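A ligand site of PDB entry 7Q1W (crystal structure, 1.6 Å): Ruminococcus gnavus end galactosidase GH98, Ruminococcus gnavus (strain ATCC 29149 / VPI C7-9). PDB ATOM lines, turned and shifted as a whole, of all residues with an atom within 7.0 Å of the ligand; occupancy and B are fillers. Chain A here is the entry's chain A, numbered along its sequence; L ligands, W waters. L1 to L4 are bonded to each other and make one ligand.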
ATOM      1  N   LEU A 470      19.415  -4.906  39.282  1.00  0.00           N
ATOM      2  CA  LEU A 470      20.396  -4.543  38.243  1.00  0.00           C
ATOM      3  C   LEU A 470      20.638  -3.028  38.265  1.00  0.00           C
ATOM      4  O   LEU A 470      19.671  -2.247  38.272  1.00  0.00           O
ATOM      5  CB  LEU A 470      19.839  -4.997  36.899  1.00  0.00           C
ATOM      6  CG  LEU A 470      20.778  -4.840  35.706  1.00  0.00           C
ATOM      7  CD1 LEU A 470      22.040  -5.656  35.859  1.00  0.00           C
ATOM      8  CD2 LEU A 470      20.065  -5.229  34.436  1.00  0.00           C
ATOM      9  N   TRP A 471      21.909  -2.640  38.329  1.00  0.00           N
ATOM     10  CA  TRP A 471      22.376  -1.221  38.294  1.00  0.00           C
ATOM     11  C   TRP A 471      22.156  -0.512  39.643  1.00  0.00           C
ATOM     12  O   TRP A 471      22.450   0.698  39.709  1.00  0.00           O
ATOM     13  CB  TRP A 471      21.679  -0.419  37.173  1.00  0.00           C
ATOM     14  CG  TRP A 471      21.603  -1.110  35.837  1.00  0.00           C
ATOM     15  CD1 TRP A 471      20.493  -1.176  35.069  1.00  0.00           C
ATOM     16  CD2 TRP A 471      22.638  -1.838  35.134  1.00  0.00           C
ATOM     17  NE1 TRP A 471      20.771  -1.855  33.906  1.00  0.00           N
ATOM     18  CE2 TRP A 471      22.081  -2.231  33.896  1.00  0.00           C
ATOM     19  CE3 TRP A 471      23.992  -2.102  35.384  1.00  0.00           C
ATOM     20  CZ2 TRP A 471      22.800  -2.985  32.953  1.00  0.00           C
ATOM     21  CZ3 TRP A 471      24.718  -2.770  34.415  1.00  0.00           C
ATOM     22  CH2 TRP A 471      24.126  -3.231  33.234  1.00  0.00           C
ATOM     23  N   ASN A 663      25.828   0.591  34.043  1.00  0.00           N
ATOM     24  CA  ASN A 663      25.461   0.241  32.656  1.00  0.00           C
ATOM     25  C   ASN A 663      26.257   1.145  31.704  1.00  0.00           C
ATOM     26  O   ASN A 663      25.716   2.165  31.251  1.00  0.00           O
ATOM     27  CB  ASN A 663      23.964   0.381  32.426  1.00  0.00           C
ATOM     28  CG  ASN A 663      23.561  -0.138  31.059  1.00  0.00           C
ATOM     29  OD1 ASN A 663      24.345  -0.784  30.370  1.00  0.00           O
ATOM     30  ND2 ASN A 663      22.327   0.119  30.682  1.00  0.00           N
ATOM     31  N   LYS A 665      28.979   0.992  28.137  1.00  0.00           N
ATOM     32  CA  LYS A 665      29.677   0.250  27.068  1.00  0.00           C
ATOM     33  C   LYS A 665      31.182   0.417  27.257  1.00  0.00           C
ATOM     34  O   LYS A 665      31.611   1.469  27.747  1.00  0.00           O
ATOM     35  CB  LYS A 665      29.294   0.777  25.670  1.00  0.00           C
ATOM     36  CG  LYS A 665      27.816   0.714  25.340  1.00  0.00           C
ATOM     37  CD  LYS A 665      27.474   1.348  23.988  1.00  0.00           C
ATOM     38  CE  LYS A 665      26.009   1.207  23.612  1.00  0.00           C
ATOM     39  NZ  LYS A 665      25.669  -0.224  23.344  1.00  0.00           N
ATOM     40  N   GLU A 686      28.448  -4.208  26.141  1.00  0.00           N
ATOM     41  CA  GLU A 686      27.730  -3.747  27.346  1.00  0.00           C
ATOM     42  C   GLU A 686      28.121  -4.682  28.484  1.00  0.00           C
ATOM     43  O   GLU A 686      28.774  -5.695  28.250  1.00  0.00           O
ATOM     44  CB  GLU A 686      26.227  -3.765  27.065  1.00  0.00           C
ATOM     45  CG  GLU A 686      25.881  -2.837  25.902  1.00  0.00           C
ATOM     46  CD  GLU A 686      24.403  -2.612  25.656  1.00  0.00           C
ATOM     47  OE1 GLU A 686      23.576  -3.024  26.533  1.00  0.00           O
ATOM     48  OE2 GLU A 686      24.069  -2.037  24.583  1.00  0.00           O
ATOM     49  N   ARG A 710      22.448 -13.398  31.200  1.00  0.00           N
ATOM     50  CA  ARG A 710      21.981 -12.682  32.409  1.00  0.00           C
ATOM     51  C   ARG A 710      20.480 -12.864  32.559  1.00  0.00           C
ATOM     52  O   ARG A 710      19.702 -12.505  31.642  1.00  0.00           O
ATOM     53  CB  ARG A 710      22.382 -11.215  32.420  1.00  0.00           C
ATOM     54  CG  ARG A 710      22.066 -10.535  33.752  1.00  0.00           C
ATOM     55  CD  ARG A 710      22.485  -9.091  33.717  1.00  0.00           C
ATOM     56  NE  ARG A 710      21.632  -8.314  32.818  1.00  0.00           N
ATOM     57  CZ  ARG A 710      22.014  -7.288  32.049  1.00  0.00           C
ATOM     58  NH1 ARG A 710      23.247  -6.803  32.141  1.00  0.00           N
ATOM     59  NH2 ARG A 710      21.129  -6.704  31.252  1.00  0.00           N
ATOM     60  N   ASN A 765      15.393 -13.094  28.284  1.00  0.00           N
ATOM     61  CA  ASN A 765      14.986 -12.851  26.872  1.00  0.00           C
ATOM     62  C   ASN A 765      15.295 -11.417  26.437  1.00  0.00           C
ATOM     63  O   ASN A 765      15.104 -11.114  25.218  1.00  0.00           O
ATOM     64  CB  ASN A 765      13.516 -13.185  26.693  1.00  0.00           C
ATOM     65  CG  ASN A 765      13.305 -14.654  26.960  1.00  0.00           C
ATOM     66  OD1 ASN A 765      14.160 -15.445  26.603  1.00  0.00           O
ATOM     67  ND2 ASN A 765      12.202 -15.016  27.597  1.00  0.00           N
ATOM     68  N   GLU A 766      15.704 -10.528  27.348  1.00  0.00           N
ATOM     69  CA  GLU A 766      16.034  -9.134  26.956  1.00  0.00           C
ATOM     70  C   GLU A 766      17.454  -9.135  26.389  1.00  0.00           C
ATOM     71  O   GLU A 766      18.396  -9.467  27.135  1.00  0.00           O
ATOM     72  CB  GLU A 766      15.907  -8.141  28.109  1.00  0.00           C
ATOM     73  CG  GLU A 766      16.045  -6.686  27.631  1.00  0.00           C
ATOM     74  CD  GLU A 766      16.107  -5.574  28.688  1.00  0.00           C
ATOM     75  OE1 GLU A 766      15.681  -5.815  29.821  1.00  0.00           O
ATOM     76  OE2 GLU A 766      16.542  -4.454  28.354  1.00  0.00           O
ATOM     77  N   LEU A 767      17.612  -8.774  25.115  1.00  0.00           N
ATOM     78  CA  LEU A 767      18.913  -8.929  24.432  1.00  0.00           C
ATOM     79  C   LEU A 767      19.733  -7.633  24.508  1.00  0.00           C
ATOM     80  O   LEU A 767      19.168  -6.513  24.606  1.00  0.00           O
ATOM     81  CB  LEU A 767      18.704  -9.355  22.987  1.00  0.00           C
ATOM     82  CG  LEU A 767      17.735 -10.508  22.752  1.00  0.00           C
ATOM     83  CD1 LEU A 767      17.685 -10.788  21.249  1.00  0.00           C
ATOM     84  CD2 LEU A 767      18.149 -11.748  23.554  1.00  0.00           C
ATOM     85  N   ARG A 768      21.054  -7.781  24.462  1.00  0.00           N
ATOM     86  CA  ARG A 768      21.962  -6.606  24.461  1.00  0.00           C
ATOM     87  C   ARG A 768      22.904  -6.685  23.271  1.00  0.00           C
ATOM     88  O   ARG A 768      23.287  -7.784  22.858  1.00  0.00           O
ATOM     89  CB  ARG A 768      22.788  -6.553  25.755  1.00  0.00           C
ATOM     90  CG  ARG A 768      21.946  -6.241  26.985  1.00  0.00           C
ATOM     91  CD  ARG A 768      21.701  -7.406  27.903  1.00  0.00           C
ATOM     92  NE  ARG A 768      22.947  -7.740  28.570  1.00  0.00           N
ATOM     93  CZ  ARG A 768      23.283  -8.922  29.016  1.00  0.00           C
ATOM     94  NH1 ARG A 768      22.459  -9.933  28.872  1.00  0.00           N
ATOM     95  NH2 ARG A 768      24.484  -9.114  29.532  1.00  0.00           N
ATOM     96  N   THR A 769      23.340  -5.514  22.823  1.00  0.00           N
ATOM     97  CA  THR A 769      24.079  -5.340  21.564  1.00  0.00           C
ATOM     98  C   THR A 769      25.580  -5.496  21.781  1.00  0.00           C
ATOM     99  O   THR A 769      26.125  -4.873  22.701  1.00  0.00           O
ATOM    100  CB  THR A 769      23.749  -3.975  20.952  1.00  0.00           C
ATOM    101  OG1 THR A 769      22.358  -4.014  20.625  1.00  0.00           O
ATOM    102  CG2 THR A 769      24.561  -3.727  19.709  1.00  0.00           C
ATOM    103  N   THR A 770      26.216  -6.298  20.917  1.00  0.00           N
ATOM    104  CA  THR A 770      27.687  -6.298  20.704  1.00  0.00           C
ATOM    105  C   THR A 770      27.958  -5.802  19.284  1.00  0.00           C
ATOM    106  O   THR A 770      27.247  -6.237  18.342  1.00  0.00           O
ATOM    107  CB  THR A 770      28.304  -7.682  20.967  1.00  0.00           C
ATOM    108  OG1 THR A 770      27.924  -8.143  22.268  1.00  0.00           O
ATOM    109  CG2 THR A 770      29.803  -7.609  20.889  1.00  0.00           C
ATOM    110  N   THR A 771      28.960  -4.944  19.124  1.00  0.00           N
ATOM    111  CA  THR A 771      29.358  -4.469  17.780  1.00  0.00           C
ATOM    112  C   THR A 771      30.850  -4.766  17.572  1.00  0.00           C
ATOM    113  O   THR A 771      31.663  -4.701  18.528  1.00  0.00           O
ATOM    114  CB  THR A 771      28.897  -3.019  17.576  1.00  0.00           C
ATOM    115  OG1 THR A 771      29.905  -2.234  18.184  1.00  0.00           O
ATOM    116  CG2 THR A 771      27.543  -2.740  18.196  1.00  0.00           C
ATOM    117  N   THR A 800      19.744 -12.651  17.914  1.00  0.00           N
ATOM    118  CA  THR A 800      19.282 -12.219  16.573  1.00  0.00           C
ATOM    119  C   THR A 800      20.391 -12.506  15.565  1.00  0.00           C
ATOM    120  O   THR A 800      21.542 -12.656  15.958  1.00  0.00           O
ATOM    121  CB  THR A 800      18.948 -10.726  16.565  1.00  0.00           C
ATOM    122  OG1 THR A 800      20.104 -10.003  16.992  1.00  0.00           O
ATOM    123  CG2 THR A 800      17.767 -10.389  17.447  1.00  0.00           C
ATOM    124  N   THR A 816      26.849  -6.081  13.810  1.00  0.00           N
ATOM    125  CA  THR A 816      26.022  -5.858  15.010  1.00  0.00           C
ATOM    126  C   THR A 816      25.306  -7.165  15.357  1.00  0.00           C
ATOM    127  O   THR A 816      24.735  -7.775  14.476  1.00  0.00           O
ATOM    128  CB  THR A 816      25.094  -4.663  14.751  1.00  0.00           C
ATOM    129  OG1 THR A 816      25.942  -3.570  14.413  1.00  0.00           O
ATOM    130  CG2 THR A 816      24.270  -4.304  15.962  1.00  0.00           C
ATOM    131  N   ILE A 817      25.268  -7.546  16.621  1.00  0.00           N
ATOM    132  CA  ILE A 817      24.446  -8.706  17.055  1.00  0.00           C
ATOM    133  C   ILE A 817      23.833  -8.377  18.420  1.00  0.00           C
ATOM    134  O   ILE A 817      24.422  -7.560  19.174  1.00  0.00           O
ATOM    135  CB  ILE A 817      25.275 -10.003  17.070  1.00  0.00           C
ATOM    136  CG1 ILE A 817      24.339 -11.202  17.159  1.00  0.00           C
ATOM    137  CG2 ILE A 817      26.310  -9.971  18.189  1.00  0.00           C
ATOM    138  CD1 ILE A 817      25.039 -12.542  17.028  1.00  0.00           C
ATOM    139  N   GLN A 818      22.660  -8.934  18.678  1.00  0.00           N
ATOM    140  CA  GLN A 818      21.949  -8.805  19.977  1.00  0.00           C
ATOM    141  C   GLN A 818      21.905 -10.206  20.590  1.00  0.00           C
ATOM    142  O   GLN A 818      21.525 -11.184  19.908  1.00  0.00           O
ATOM    143  CB  GLN A 818      20.542  -8.245  19.812  1.00  0.00           C
ATOM    144  CG  GLN A 818      20.504  -6.850  19.209  1.00  0.00           C
ATOM    145  CD  GLN A 818      19.337  -6.127  19.833  1.00  0.00           C
ATOM    146  OE1 GLN A 818      19.503  -5.298  20.742  1.00  0.00           O
ATOM    147  NE2 GLN A 818      18.140  -6.562  19.472  1.00  0.00           N
HETATM  148  C1  LIG L   1       9.855  -2.519  20.448  1.00  0.00           C
HETATM  149  C2  LIG L   1      10.533  -1.364  19.711  1.00  0.00           C
HETATM  150  C3  LIG L   1      12.049  -1.522  19.787  1.00  0.00           C
HETATM  151  C4  LIG L   1      12.463  -1.683  21.246  1.00  0.00           C
HETATM  152  C5  LIG L   1      11.726  -2.872  21.869  1.00  0.00           C
HETATM  153  C6  LIG L   1      12.051  -3.086  23.328  1.00  0.00           C
HETATM  154  C7  LIG L   1       9.539  -0.121  17.839  1.00  0.00           C
HETATM  155  C8  LIG L   1       8.753  -0.285  16.570  1.00  0.00           C
HETATM  156  N1  LIG L   1      10.112  -1.223  18.327  1.00  0.00           N
HETATM  157  O1  LIG L   1       8.477  -2.310  20.461  1.00  0.00           O
HETATM  158  O2  LIG L   1      12.686  -0.389  19.215  1.00  0.00           O
HETATM  159  O3  LIG L   1      13.877  -1.917  21.296  1.00  0.00           O
HETATM  160  O4  LIG L   1      10.310  -2.628  21.788  1.00  0.00           O
HETATM  161  O5  LIG L   1      11.775  -1.925  24.105  1.00  0.00           O
HETATM  162  O6  LIG L   1       9.665   0.967  18.382  1.00  0.00           O
HETATM  163  C1  LG2 L   2      14.640  -1.098  22.134  1.00  0.00           C
HETATM  164  C2  LG2 L   2      16.019  -1.741  22.293  1.00  0.00           C
HETATM  165  C3  LG2 L   2      16.903  -0.835  23.148  1.00  0.00           C
HETATM  166  C4  LG2 L   2      16.964   0.575  22.564  1.00  0.00           C
HETATM  167  C5  LG2 L   2      15.562   1.120  22.337  1.00  0.00           C
HETATM  168  C6  LG2 L   2      15.568   2.447  21.603  1.00  0.00           C
HETATM  169  O1  LG2 L   2      15.895  -3.040  22.894  1.00  0.00           O
HETATM  170  O2  LG2 L   2      18.235  -1.370  23.169  1.00  0.00           O
HETATM  171  O3  LG2 L   2      17.674   0.552  21.329  1.00  0.00           O
HETATM  172  O4  LG2 L   2      14.774   0.199  21.555  1.00  0.00           O
HETATM  173  O5  LG2 L   2      14.247   2.927  21.391  1.00  0.00           O
HETATM  174  C1  LG3 L   3      16.704  -4.048  22.312  1.00  0.00           C
HETATM  175  C2  LG3 L   3      16.698  -5.312  23.167  1.00  0.00           C
HETATM  176  C3  LG3 L   3      15.392  -6.128  23.035  1.00  0.00           C
HETATM  177  C4  LG3 L   3      14.996  -6.290  21.564  1.00  0.00           C
HETATM  178  C5  LG3 L   3      14.970  -4.928  20.873  1.00  0.00           C
HETATM  179  C6  LG3 L   3      14.644  -5.004  19.401  1.00  0.00           C
HETATM  180  O1  LG3 L   3      16.947  -4.948  24.523  1.00  0.00           O
HETATM  181  O2  LG3 L   3      15.526  -7.421  23.646  1.00  0.00           O
HETATM  182  O3  LG3 L   3      15.914  -7.156  20.892  1.00  0.00           O
HETATM  183  O4  LG3 L   3      16.283  -4.322  20.975  1.00  0.00           O
HETATM  184  O1  LG4 L   4      18.782  -1.092  25.422  1.00  0.00           O
HETATM  185  C1  LG4 L   4      19.146  -0.790  24.070  1.00  0.00           C
HETATM  186  C2  LG4 L   4      20.529  -1.274  23.708  1.00  0.00           C
HETATM  187  N1  LG4 L   4      20.878  -0.990  22.321  1.00  0.00           N
HETATM  188  C3  LG4 L   4      20.652  -2.760  24.043  1.00  0.00           C
HETATM  189  O2  LG4 L   4      21.986  -3.191  23.778  1.00  0.00           O
HETATM  190  C4  LG4 L   4      20.279  -3.004  25.502  1.00  0.00           C
HETATM  191  O3  LG4 L   4      21.171  -2.315  26.372  1.00  0.00           O
HETATM  192  C5  LG4 L   4      18.870  -2.490  25.765  1.00  0.00           C
HETATM  193  C6  LG4 L   4      18.473  -2.607  27.219  1.00  0.00           C
HETATM  194  O4  LG4 L   4      18.926  -3.849  27.788  1.00  0.00           O
HETATM  195  C7  LG4 L   4      21.999  -0.382  21.910  1.00  0.00           C
HETATM  196  O5  LG4 L   4      22.898  -0.046  22.685  1.00  0.00           O
HETATM  197  C8  LG4 L   4      22.126  -0.149  20.436  1.00  0.00           C
HETATM  198  O   HOH W   1      15.367  -3.724  25.916  1.00  0.00           O
HETATM  199  O   HOH W   2      21.045  -4.123  29.858  1.00  0.00           O
HETATM  200  O   HOH W   3      21.110  -0.362  28.110  1.00  0.00           O
HETATM  201  O   HOH W   4      22.208  -1.946  17.636  1.00  0.00           O
HETATM  202  O   HOH W   5      18.942  -1.466  20.099  1.00  0.00           O
HETATM  203  O   HOH W   6      18.094  -0.565  30.023  1.00  0.00           O
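An oxygen (O5) of LG4 L4 sits at hydrogen-bond distance from the side-chain amino group of Lys 665 (2.9 Å).
The side-chain carboxylate of Glu 766 lies within hydrogen-bond range of an oxygen (O4) of LG4 L4 (2.5 Å).
The backbone NH (N) of Thr 769 sits at hydrogen-bond distance from an oxygen (O2) of LG4 L4 (2.9 Å).
An oxygen (O3) of LG3 L3 sits at hydrogen-bond distance from the side-chain amide nitrogen (NE2) of Gln 818 (2.7 Å).
An oxygen (O3) of LG4 L4 lies within hydrogen-bond range of the side-chain carboxylate (OE1) of Glu 686, 2.5 Å away.
The backbone carbonyl oxygen of Leu 767 lies within hydrogen-bond range of an oxygen (O1) of LG3 L3, at 2.7 Å.
N of Leu 767 is in hydrogen-bond range of O2 of LG3 L3.
An oxygen (O2) of LG4 L4 sits at hydrogen-bond distance from the side-chain hydroxyl (OG1) of Thr 769 (3.3 Å).
OG1 of Thr 769 is in hydrogen-bond range of OE1 of Gln 818 (3.1 Å).
The side-chain amino group (NZ) of Lys 665 is in salt-bridge range of the side-chain carboxylate (OE2) of Glu 686 (2.7 Å).
The backbone carbonyl oxygen of Gln 818 is in hydrogen-bond range of the backbone NH of Thr 800 (3.0 Å).
CA of Arg 768 touches O2 of LG4 L4, 3.5 Å away.
Hydrophobic or aromatic side chains within 4 Å of the ligand: Leu 767.
Water W1 lies within hydrogen-bond range of an oxygen (O1) of LG3 L3 (2.4 Å) and the side-chain carboxylate of Glu 766 (2.8 Å).
Water W3 lies within hydrogen-bond range of O3 of LG4 L4 (2.6 Å) and ND2 of Asn 663 (2.9 Å).
Water W2 bridges the guanidinium group (NH2) of Arg 710 (2.9 Å) and an oxygen (O4) of LG4 L4 (3.0 Å).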
